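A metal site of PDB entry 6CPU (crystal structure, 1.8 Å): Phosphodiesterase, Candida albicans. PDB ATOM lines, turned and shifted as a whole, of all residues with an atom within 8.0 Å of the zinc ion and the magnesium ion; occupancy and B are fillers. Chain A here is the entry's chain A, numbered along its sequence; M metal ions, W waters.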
ATOM      1  N   TYR A 267       7.959  13.049  -1.968  1.00  0.00           N
ATOM      2  CA  TYR A 267       9.120  12.428  -2.605  1.00  0.00           C
ATOM      3  C   TYR A 267      10.381  13.150  -2.189  1.00  0.00           C
ATOM      4  O   TYR A 267      10.369  14.363  -2.020  1.00  0.00           O
ATOM      5  CB  TYR A 267       8.944  12.405  -4.138  1.00  0.00           C
ATOM      6  CG  TYR A 267       8.025  11.303  -4.601  1.00  0.00           C
ATOM      7  CD1 TYR A 267       6.678  11.534  -4.847  1.00  0.00           C
ATOM      8  CD2 TYR A 267       8.511  10.010  -4.787  1.00  0.00           C
ATOM      9  CE1 TYR A 267       5.837  10.498  -5.236  1.00  0.00           C
ATOM     10  CE2 TYR A 267       7.664   8.980  -5.180  1.00  0.00           C
ATOM     11  CZ  TYR A 267       6.326   9.221  -5.408  1.00  0.00           C
ATOM     12  OH  TYR A 267       5.503   8.162  -5.806  1.00  0.00           O
ATOM     13  N   PHE A 273      17.486   8.318  -7.884  1.00  0.00           N
ATOM     14  CA  PHE A 273      16.521   7.564  -8.677  1.00  0.00           C
ATOM     15  C   PHE A 273      15.071   7.640  -8.187  1.00  0.00           C
ATOM     16  O   PHE A 273      14.205   8.032  -8.956  1.00  0.00           O
ATOM     17  CB  PHE A 273      16.930   6.097  -8.758  1.00  0.00           C
ATOM     18  CG  PHE A 273      16.079   5.300  -9.693  1.00  0.00           C
ATOM     19  CD1 PHE A 273      16.437   5.176 -11.020  1.00  0.00           C
ATOM     20  CD2 PHE A 273      14.923   4.672  -9.259  1.00  0.00           C
ATOM     21  CE1 PHE A 273      15.671   4.441 -11.893  1.00  0.00           C
ATOM     22  CE2 PHE A 273      14.136   3.946 -10.136  1.00  0.00           C
ATOM     23  CZ  PHE A 273      14.522   3.817 -11.464  1.00  0.00           C
ATOM     24  N   HIS A 274      14.828   7.216  -6.942  1.00  0.00           N
ATOM     25  CA  HIS A 274      13.467   7.141  -6.381  1.00  0.00           C
ATOM     26  C   HIS A 274      12.934   8.491  -5.902  1.00  0.00           C
ATOM     27  O   HIS A 274      12.681   8.699  -4.720  1.00  0.00           O
ATOM     28  CB  HIS A 274      13.405   6.101  -5.264  1.00  0.00           C
ATOM     29  CG  HIS A 274      13.563   4.700  -5.770  1.00  0.00           C
ATOM     30  ND1 HIS A 274      14.760   4.016  -5.729  1.00  0.00           N
ATOM     31  CD2 HIS A 274      12.683   3.870  -6.376  1.00  0.00           C
ATOM     32  CE1 HIS A 274      14.602   2.817  -6.268  1.00  0.00           C
ATOM     33  NE2 HIS A 274      13.347   2.708  -6.669  1.00  0.00           N
ATOM     34  N   ASN A 275      12.771   9.397  -6.851  1.00  0.00           N
ATOM     35  CA  ASN A 275      12.293  10.760  -6.594  1.00  0.00           C
ATOM     36  C   ASN A 275      11.002  10.983  -7.355  1.00  0.00           C
ATOM     37  O   ASN A 275      10.423  10.042  -7.906  1.00  0.00           O
ATOM     38  CB  ASN A 275      13.359  11.773  -6.967  1.00  0.00           C
ATOM     39  CG  ASN A 275      13.828  11.614  -8.401  1.00  0.00           C
ATOM     40  OD1 ASN A 275      13.118  11.106  -9.249  1.00  0.00           O
ATOM     41  ND2 ASN A 275      15.034  12.022  -8.649  1.00  0.00           N
ATOM     42  N   HIS A 278      10.919   9.851 -11.055  1.00  0.00           N
ATOM     43  CA  HIS A 278      10.653   8.408 -11.241  1.00  0.00           C
ATOM     44  C   HIS A 278       9.161   8.118 -11.166  1.00  0.00           C
ATOM     45  O   HIS A 278       8.632   7.370 -11.986  1.00  0.00           O
ATOM     46  CB  HIS A 278      11.421   7.545 -10.216  1.00  0.00           C
ATOM     47  CG  HIS A 278      10.988   6.106 -10.174  1.00  0.00           C
ATOM     48  ND1 HIS A 278      11.115   5.246 -11.254  1.00  0.00           N
ATOM     49  CD2 HIS A 278      10.441   5.366  -9.177  1.00  0.00           C
ATOM     50  CE1 HIS A 278      10.657   4.047 -10.915  1.00  0.00           C
ATOM     51  NE2 HIS A 278      10.241   4.097  -9.659  1.00  0.00           N
ATOM     52  N   ALA A 279       8.480   8.704 -10.173  1.00  0.00           N
ATOM     53  CA  ALA A 279       7.051   8.522 -10.035  1.00  0.00           C
ATOM     54  C   ALA A 279       6.299   8.957 -11.298  1.00  0.00           C
ATOM     55  O   ALA A 279       5.395   8.254 -11.784  1.00  0.00           O
ATOM     56  CB  ALA A 279       6.522   9.286  -8.835  1.00  0.00           C
ATOM     57  N   VAL A 282       6.955   6.550 -14.190  1.00  0.00           N
ATOM     58  CA  VAL A 282       6.127   5.349 -14.052  1.00  0.00           C
ATOM     59  C   VAL A 282       4.667   5.624 -14.382  1.00  0.00           C
ATOM     60  O   VAL A 282       3.987   4.812 -15.053  1.00  0.00           O
ATOM     61  CB  VAL A 282       6.271   4.716 -12.633  1.00  0.00           C
ATOM     62  CG1 VAL A 282       5.271   3.590 -12.421  1.00  0.00           C
ATOM     63  CG2 VAL A 282       7.681   4.199 -12.417  1.00  0.00           C
ATOM     64  N   ALA A 346       0.220   4.551  -9.678  1.00  0.00           N
ATOM     65  CA  ALA A 346       1.552   4.756 -10.211  1.00  0.00           C
ATOM     66  C   ALA A 346       2.168   6.059  -9.677  1.00  0.00           C
ATOM     67  O   ALA A 346       3.347   6.098  -9.316  1.00  0.00           O
ATOM     68  CB  ALA A 346       1.512   4.779 -11.749  1.00  0.00           C
ATOM     69  N   GLY A 348       1.653   7.481  -6.798  1.00  0.00           N
ATOM     70  CA  GLY A 348       1.993   7.354  -5.378  1.00  0.00           C
ATOM     71  C   GLY A 348       2.838   6.150  -5.002  1.00  0.00           C
ATOM     72  O   GLY A 348       3.138   5.931  -3.818  1.00  0.00           O
ATOM     73  N   HIS A 349       3.262   5.371  -5.996  1.00  0.00           N
ATOM     74  CA  HIS A 349       3.774   4.022  -5.689  1.00  0.00           C
ATOM     75  C   HIS A 349       5.099   3.980  -4.925  1.00  0.00           C
ATOM     76  O   HIS A 349       5.410   2.949  -4.321  1.00  0.00           O
ATOM     77  CB  HIS A 349       3.868   3.160  -6.971  1.00  0.00           C
ATOM     78  CG  HIS A 349       5.180   3.297  -7.681  1.00  0.00           C
ATOM     79  ND1 HIS A 349       5.486   4.367  -8.478  1.00  0.00           N
ATOM     80  CD2 HIS A 349       6.281   2.510  -7.672  1.00  0.00           C
ATOM     81  CE1 HIS A 349       6.716   4.238  -8.936  1.00  0.00           C
ATOM     82  NE2 HIS A 349       7.220   3.109  -8.463  1.00  0.00           N
ATOM     83  N   ASP A 350       5.875   5.068  -4.940  1.00  0.00           N
ATOM     84  CA  ASP A 350       7.125   5.151  -4.193  1.00  0.00           C
ATOM     85  C   ASP A 350       7.137   6.297  -3.171  1.00  0.00           C
ATOM     86  O   ASP A 350       8.198   6.736  -2.775  1.00  0.00           O
ATOM     87  CB  ASP A 350       8.316   5.300  -5.175  1.00  0.00           C
ATOM     88  CG  ASP A 350       8.861   3.953  -5.690  1.00  0.00           C
ATOM     89  OD1 ASP A 350       8.741   2.956  -4.955  1.00  0.00           O
ATOM     90  OD2 ASP A 350       9.451   3.913  -6.799  1.00  0.00           O
ATOM     91  N   VAL A 351       5.967   6.800  -2.763  1.00  0.00           N
ATOM     92  CA  VAL A 351       5.938   7.951  -1.844  1.00  0.00           C
ATOM     93  C   VAL A 351       6.812   7.721  -0.608  1.00  0.00           C
ATOM     94  O   VAL A 351       6.757   6.671   0.036  1.00  0.00           O
ATOM     95  CB  VAL A 351       4.529   8.418  -1.402  1.00  0.00           C
ATOM     96  CG1 VAL A 351       3.762   9.046  -2.560  1.00  0.00           C
ATOM     97  CG2 VAL A 351       3.741   7.303  -0.767  1.00  0.00           C
ATOM     98  N   HIS A 353       9.987   7.365  -0.354  1.00  0.00           N
ATOM     99  CA  HIS A 353      11.091   6.421  -0.533  1.00  0.00           C
ATOM    100  C   HIS A 353      12.369   7.077  -0.032  1.00  0.00           C
ATOM    101  O   HIS A 353      12.647   8.188  -0.416  1.00  0.00           O
ATOM    102  CB  HIS A 353      11.192   6.026  -2.016  1.00  0.00           C
ATOM    103  CG  HIS A 353      12.029   4.814  -2.292  1.00  0.00           C
ATOM    104  ND1 HIS A 353      13.375   4.774  -2.047  1.00  0.00           N
ATOM    105  CD2 HIS A 353      11.721   3.630  -2.859  1.00  0.00           C
ATOM    106  CE1 HIS A 353      13.862   3.606  -2.415  1.00  0.00           C
ATOM    107  NE2 HIS A 353      12.883   2.882  -2.906  1.00  0.00           N
ATOM    108  N   THR A 356      16.879   3.808  -0.348  1.00  0.00           N
ATOM    109  CA  THR A 356      17.513   2.507  -0.046  1.00  0.00           C
ATOM    110  C   THR A 356      16.814   1.364  -0.813  1.00  0.00           C
ATOM    111  O   THR A 356      16.297   1.576  -1.897  1.00  0.00           O
ATOM    112  CB  THR A 356      17.576   2.257   1.481  1.00  0.00           C
ATOM    113  OG1 THR A 356      16.250   2.193   2.008  1.00  0.00           O
ATOM    114  CG2 THR A 356      18.306   3.345   2.183  1.00  0.00           C
ATOM    115  N   ASN A 358      14.723  -2.783  -0.113  1.00  0.00           N
ATOM    116  CA  ASN A 358      14.215  -3.737   0.886  1.00  0.00           C
ATOM    117  C   ASN A 358      15.355  -4.544   1.496  1.00  0.00           C
ATOM    118  O   ASN A 358      15.427  -4.711   2.718  1.00  0.00           O
ATOM    119  CB  ASN A 358      13.124  -4.656   0.317  1.00  0.00           C
ATOM    120  CG  ASN A 358      11.779  -3.972   0.189  1.00  0.00           C
ATOM    121  OD1 ASN A 358      11.512  -2.980   0.854  1.00  0.00           O
ATOM    122  ND2 ASN A 358      10.915  -4.503  -0.661  1.00  0.00           N
ATOM    123  N   LEU A 378       9.348  -1.523   2.084  1.00  0.00           N
ATOM    124  CA  LEU A 378       9.185  -0.188   1.535  1.00  0.00           C
ATOM    125  C   LEU A 378       7.826  -0.028   0.873  1.00  0.00           C
ATOM    126  O   LEU A 378       7.193   1.013   1.022  1.00  0.00           O
ATOM    127  CB  LEU A 378      10.331   0.176   0.580  1.00  0.00           C
ATOM    128  CG  LEU A 378      11.704   0.350   1.246  1.00  0.00           C
ATOM    129  CD1 LEU A 378      12.785   0.601   0.205  1.00  0.00           C
ATOM    130  CD2 LEU A 378      11.683   1.457   2.288  1.00  0.00           C
ATOM    131  N   GLU A 379       7.333  -1.073   0.208  1.00  0.00           N
ATOM    132  CA  GLU A 379       6.063  -0.972  -0.499  1.00  0.00           C
ATOM    133  C   GLU A 379       4.885  -0.840   0.488  1.00  0.00           C
ATOM    134  O   GLU A 379       3.887  -0.168   0.205  1.00  0.00           O
ATOM    135  CB  GLU A 379       5.848  -2.170  -1.432  1.00  0.00           C
ATOM    136  CG  GLU A 379       6.851  -2.257  -2.580  1.00  0.00           C
ATOM    137  CD  GLU A 379       8.212  -2.830  -2.201  1.00  0.00           C
ATOM    138  OE1 GLU A 379       8.371  -3.393  -1.088  1.00  0.00           O
ATOM    139  OE2 GLU A 379       9.157  -2.716  -3.015  1.00  0.00           O
ATOM    140  N   HIS A 382       5.039   2.787   1.464  1.00  0.00           N
ATOM    141  CA  HIS A 382       4.494   3.663   0.420  1.00  0.00           C
ATOM    142  C   HIS A 382       2.969   3.618   0.398  1.00  0.00           C
ATOM    143  O   HIS A 382       2.320   4.649   0.291  1.00  0.00           O
ATOM    144  CB  HIS A 382       4.985   3.313  -1.002  1.00  0.00           C
ATOM    145  CG  HIS A 382       6.463   3.192  -1.132  1.00  0.00           C
ATOM    146  ND1 HIS A 382       7.350   4.095  -0.592  1.00  0.00           N
ATOM    147  CD2 HIS A 382       7.213   2.253  -1.751  1.00  0.00           C
ATOM    148  CE1 HIS A 382       8.582   3.721  -0.871  1.00  0.00           C
ATOM    149  NE2 HIS A 382       8.528   2.598  -1.562  1.00  0.00           N
ATOM    150  N   ILE A 419       0.146  -0.924  -5.531  1.00  0.00           N
ATOM    151  CA  ILE A 419       1.383  -0.491  -4.910  1.00  0.00           C
ATOM    152  C   ILE A 419       2.149  -1.678  -4.326  1.00  0.00           C
ATOM    153  O   ILE A 419       3.373  -1.796  -4.538  1.00  0.00           O
ATOM    154  CB  ILE A 419       1.155   0.628  -3.883  1.00  0.00           C
ATOM    155  CG1 ILE A 419       0.655   1.887  -4.620  1.00  0.00           C
ATOM    156  CG2 ILE A 419       2.459   0.944  -3.162  1.00  0.00           C
ATOM    157  CD1 ILE A 419       0.351   3.080  -3.732  1.00  0.00           C
ATOM    158  N   THR A 422       4.401  -3.874  -6.625  1.00  0.00           N
ATOM    159  CA  THR A 422       5.712  -3.438  -7.124  1.00  0.00           C
ATOM    160  C   THR A 422       6.906  -3.985  -6.345  1.00  0.00           C
ATOM    161  O   THR A 422       8.038  -3.699  -6.698  1.00  0.00           O
ATOM    162  CB  THR A 422       5.841  -1.907  -7.201  1.00  0.00           C
ATOM    163  OG1 THR A 422       5.776  -1.345  -5.880  1.00  0.00           O
ATOM    164  CG2 THR A 422       4.726  -1.324  -8.066  1.00  0.00           C
ATOM    165  N   ASP A 423       6.653  -4.749  -5.281  1.00  0.00           N
ATOM    166  CA  ASP A 423       7.696  -5.437  -4.525  1.00  0.00           C
ATOM    167  C   ASP A 423       8.337  -6.550  -5.364  1.00  0.00           C
ATOM    168  O   ASP A 423       7.685  -7.545  -5.673  1.00  0.00           O
ATOM    169  CB  ASP A 423       7.091  -6.045  -3.254  1.00  0.00           C
ATOM    170  CG  ASP A 423       8.117  -6.791  -2.399  1.00  0.00           C
ATOM    171  OD1 ASP A 423       9.323  -6.631  -2.630  1.00  0.00           O
ATOM    172  OD2 ASP A 423       7.697  -7.518  -1.475  1.00  0.00           O
ATOM    173  N   MET A 424       9.599  -6.361  -5.698  1.00  0.00           N
ATOM    174  CA  MET A 424      10.317  -7.326  -6.552  1.00  0.00           C
ATOM    175  C   MET A 424      10.604  -8.656  -5.855  1.00  0.00           C
ATOM    176  O   MET A 424      10.855  -9.653  -6.526  1.00  0.00           O
ATOM    177  CB  MET A 424      11.608  -6.714  -7.104  1.00  0.00           C
ATOM    178  CG  MET A 424      11.356  -5.678  -8.192  1.00  0.00           C
ATOM    179  SD  MET A 424      10.560  -6.335  -9.672  1.00  0.00           S
ATOM    180  CE  MET A 424      11.965  -7.129 -10.473  1.00  0.00           C
ATOM    181  N   ILE A 458       1.322  -1.919 -13.558  1.00  0.00           N
ATOM    182  CA  ILE A 458       2.172  -1.097 -12.695  1.00  0.00           C
ATOM    183  C   ILE A 458       3.546  -1.742 -12.540  1.00  0.00           C
ATOM    184  O   ILE A 458       4.532  -1.046 -12.500  1.00  0.00           O
ATOM    185  CB  ILE A 458       1.494  -0.782 -11.327  1.00  0.00           C
ATOM    186  CG1 ILE A 458       2.182   0.423 -10.656  1.00  0.00           C
ATOM    187  CG2 ILE A 458       1.499  -2.013 -10.422  1.00  0.00           C
ATOM    188  CD1 ILE A 458       1.469   0.884  -9.398  1.00  0.00           C
ATOM    189  N   ALA A 461       5.386  -0.852 -15.763  1.00  0.00           N
ATOM    190  CA  ALA A 461       5.717   0.585 -15.690  1.00  0.00           C
ATOM    191  C   ALA A 461       6.879   0.869 -14.753  1.00  0.00           C
ATOM    192  O   ALA A 461       7.806   1.609 -15.095  1.00  0.00           O
ATOM    193  CB  ALA A 461       4.491   1.378 -15.257  1.00  0.00           C
ATOM    194  N   ASP A 462       6.854   0.256 -13.574  1.00  0.00           N
ATOM    195  CA  ASP A 462       7.918   0.487 -12.587  1.00  0.00           C
ATOM    196  C   ASP A 462       9.302   0.064 -13.086  1.00  0.00           C
ATOM    197  O   ASP A 462      10.302   0.693 -12.735  1.00  0.00           O
ATOM    198  CB  ASP A 462       7.577  -0.229 -11.286  1.00  0.00           C
ATOM    199  CG  ASP A 462       8.466   0.209 -10.127  1.00  0.00           C
ATOM    200  OD1 ASP A 462       8.870   1.403 -10.028  1.00  0.00           O
ATOM    201  OD2 ASP A 462       8.732  -0.679  -9.295  1.00  0.00           O
ATOM    202  N   ILE A 463       9.377  -1.007 -13.893  1.00  0.00           N
ATOM    203  CA  ILE A 463      10.668  -1.471 -14.417  1.00  0.00           C
ATOM    204  C   ILE A 463      10.823  -1.163 -15.905  1.00  0.00           C
ATOM    205  O   ILE A 463      11.520  -1.886 -16.630  1.00  0.00           O
ATOM    206  CB  ILE A 463      10.912  -2.984 -14.125  1.00  0.00           C
ATOM    207  CG1 ILE A 463       9.909  -3.878 -14.845  1.00  0.00           C
ATOM    208  CG2 ILE A 463      10.870  -3.256 -12.626  1.00  0.00           C
ATOM    209  CD1 ILE A 463      10.397  -5.300 -15.023  1.00  0.00           C
HETATM  210 ZN    ZN M   1       9.315   2.581  -8.386  1.00  0.00          ZN
HETATM  211 MG    MG M   2       9.136   0.842  -5.102  1.00  0.00          MG
HETATM  212  O   HOH W   1       7.181   0.699  -4.741  1.00  0.00           O
HETATM  213  O   HOH W   2       8.857   0.882  -7.117  1.00  0.00           O
HETATM  214  O   HOH W   3       9.802   0.730  -3.017  1.00  0.00           O
HETATM  215  O   HOH W   4      11.111   1.001  -5.409  1.00  0.00           O
HETATM  216  O   HOH W   5      11.396   1.844  -8.269  1.00  0.00           O
HETATM  217  O   HOH W   6       9.206  -1.338  -5.255  1.00  0.00           O
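The magnesium ion is bound by water W1, water W4, water W2, the side-chain carboxylate of Asp 350, water W6 and water W3.
The zinc ion is bound by OD1 of Asp 462 (2.1 Å), OD2 of Asp 350 (2.1 Å), NE2 of His 349 (2.2 Å), water W2 (2.2 Å), NE2 of His 278 (2.2 Å) and water W5 (2.2 Å).
His 382 touches the magnesium ion.
Of the 26 residues printed, 2 come within 4 Å of the magnesium ion.
The nearest printed residue that does not touch the magnesium ion is Thr 422 (4.1 Å).
The nearest printed residue that does not touch the zinc ion is His 274 (4.1 Å).
The backbone NH (N) of His 278 is in hydrogen-bond range of the side-chain amide oxygen (OD1) of Asn 275 (3.1 Å).
ND1 of His 382 sits at hydrogen-bond distance from O of Val 351 (2.7 Å).
A ring nitrogen (NE2) of His 382 sits close to the backbone carbonyl oxygen of Leu 378.
N of Asp 350 is in hydrogen-bond range of OH of Tyr 267.
NE2 of His 382 sits close to OD1 of Asp 350 (3.4 Å).
A ring nitrogen (ND1) of His 349 is in hydrogen-bond range of the backbone carbonyl oxygen (O) of Ala 346.
Water W6 lies within hydrogen-bond range of the side-chain carboxylate of Glu 379 (2.6 Å) and the backbone carbonyl oxygen of Thr 422 (3.0 Å).
Water W1 lies within hydrogen-bond range of OG1 of Thr 422 (2.7 Å) and O of His 349 (2.9 Å).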
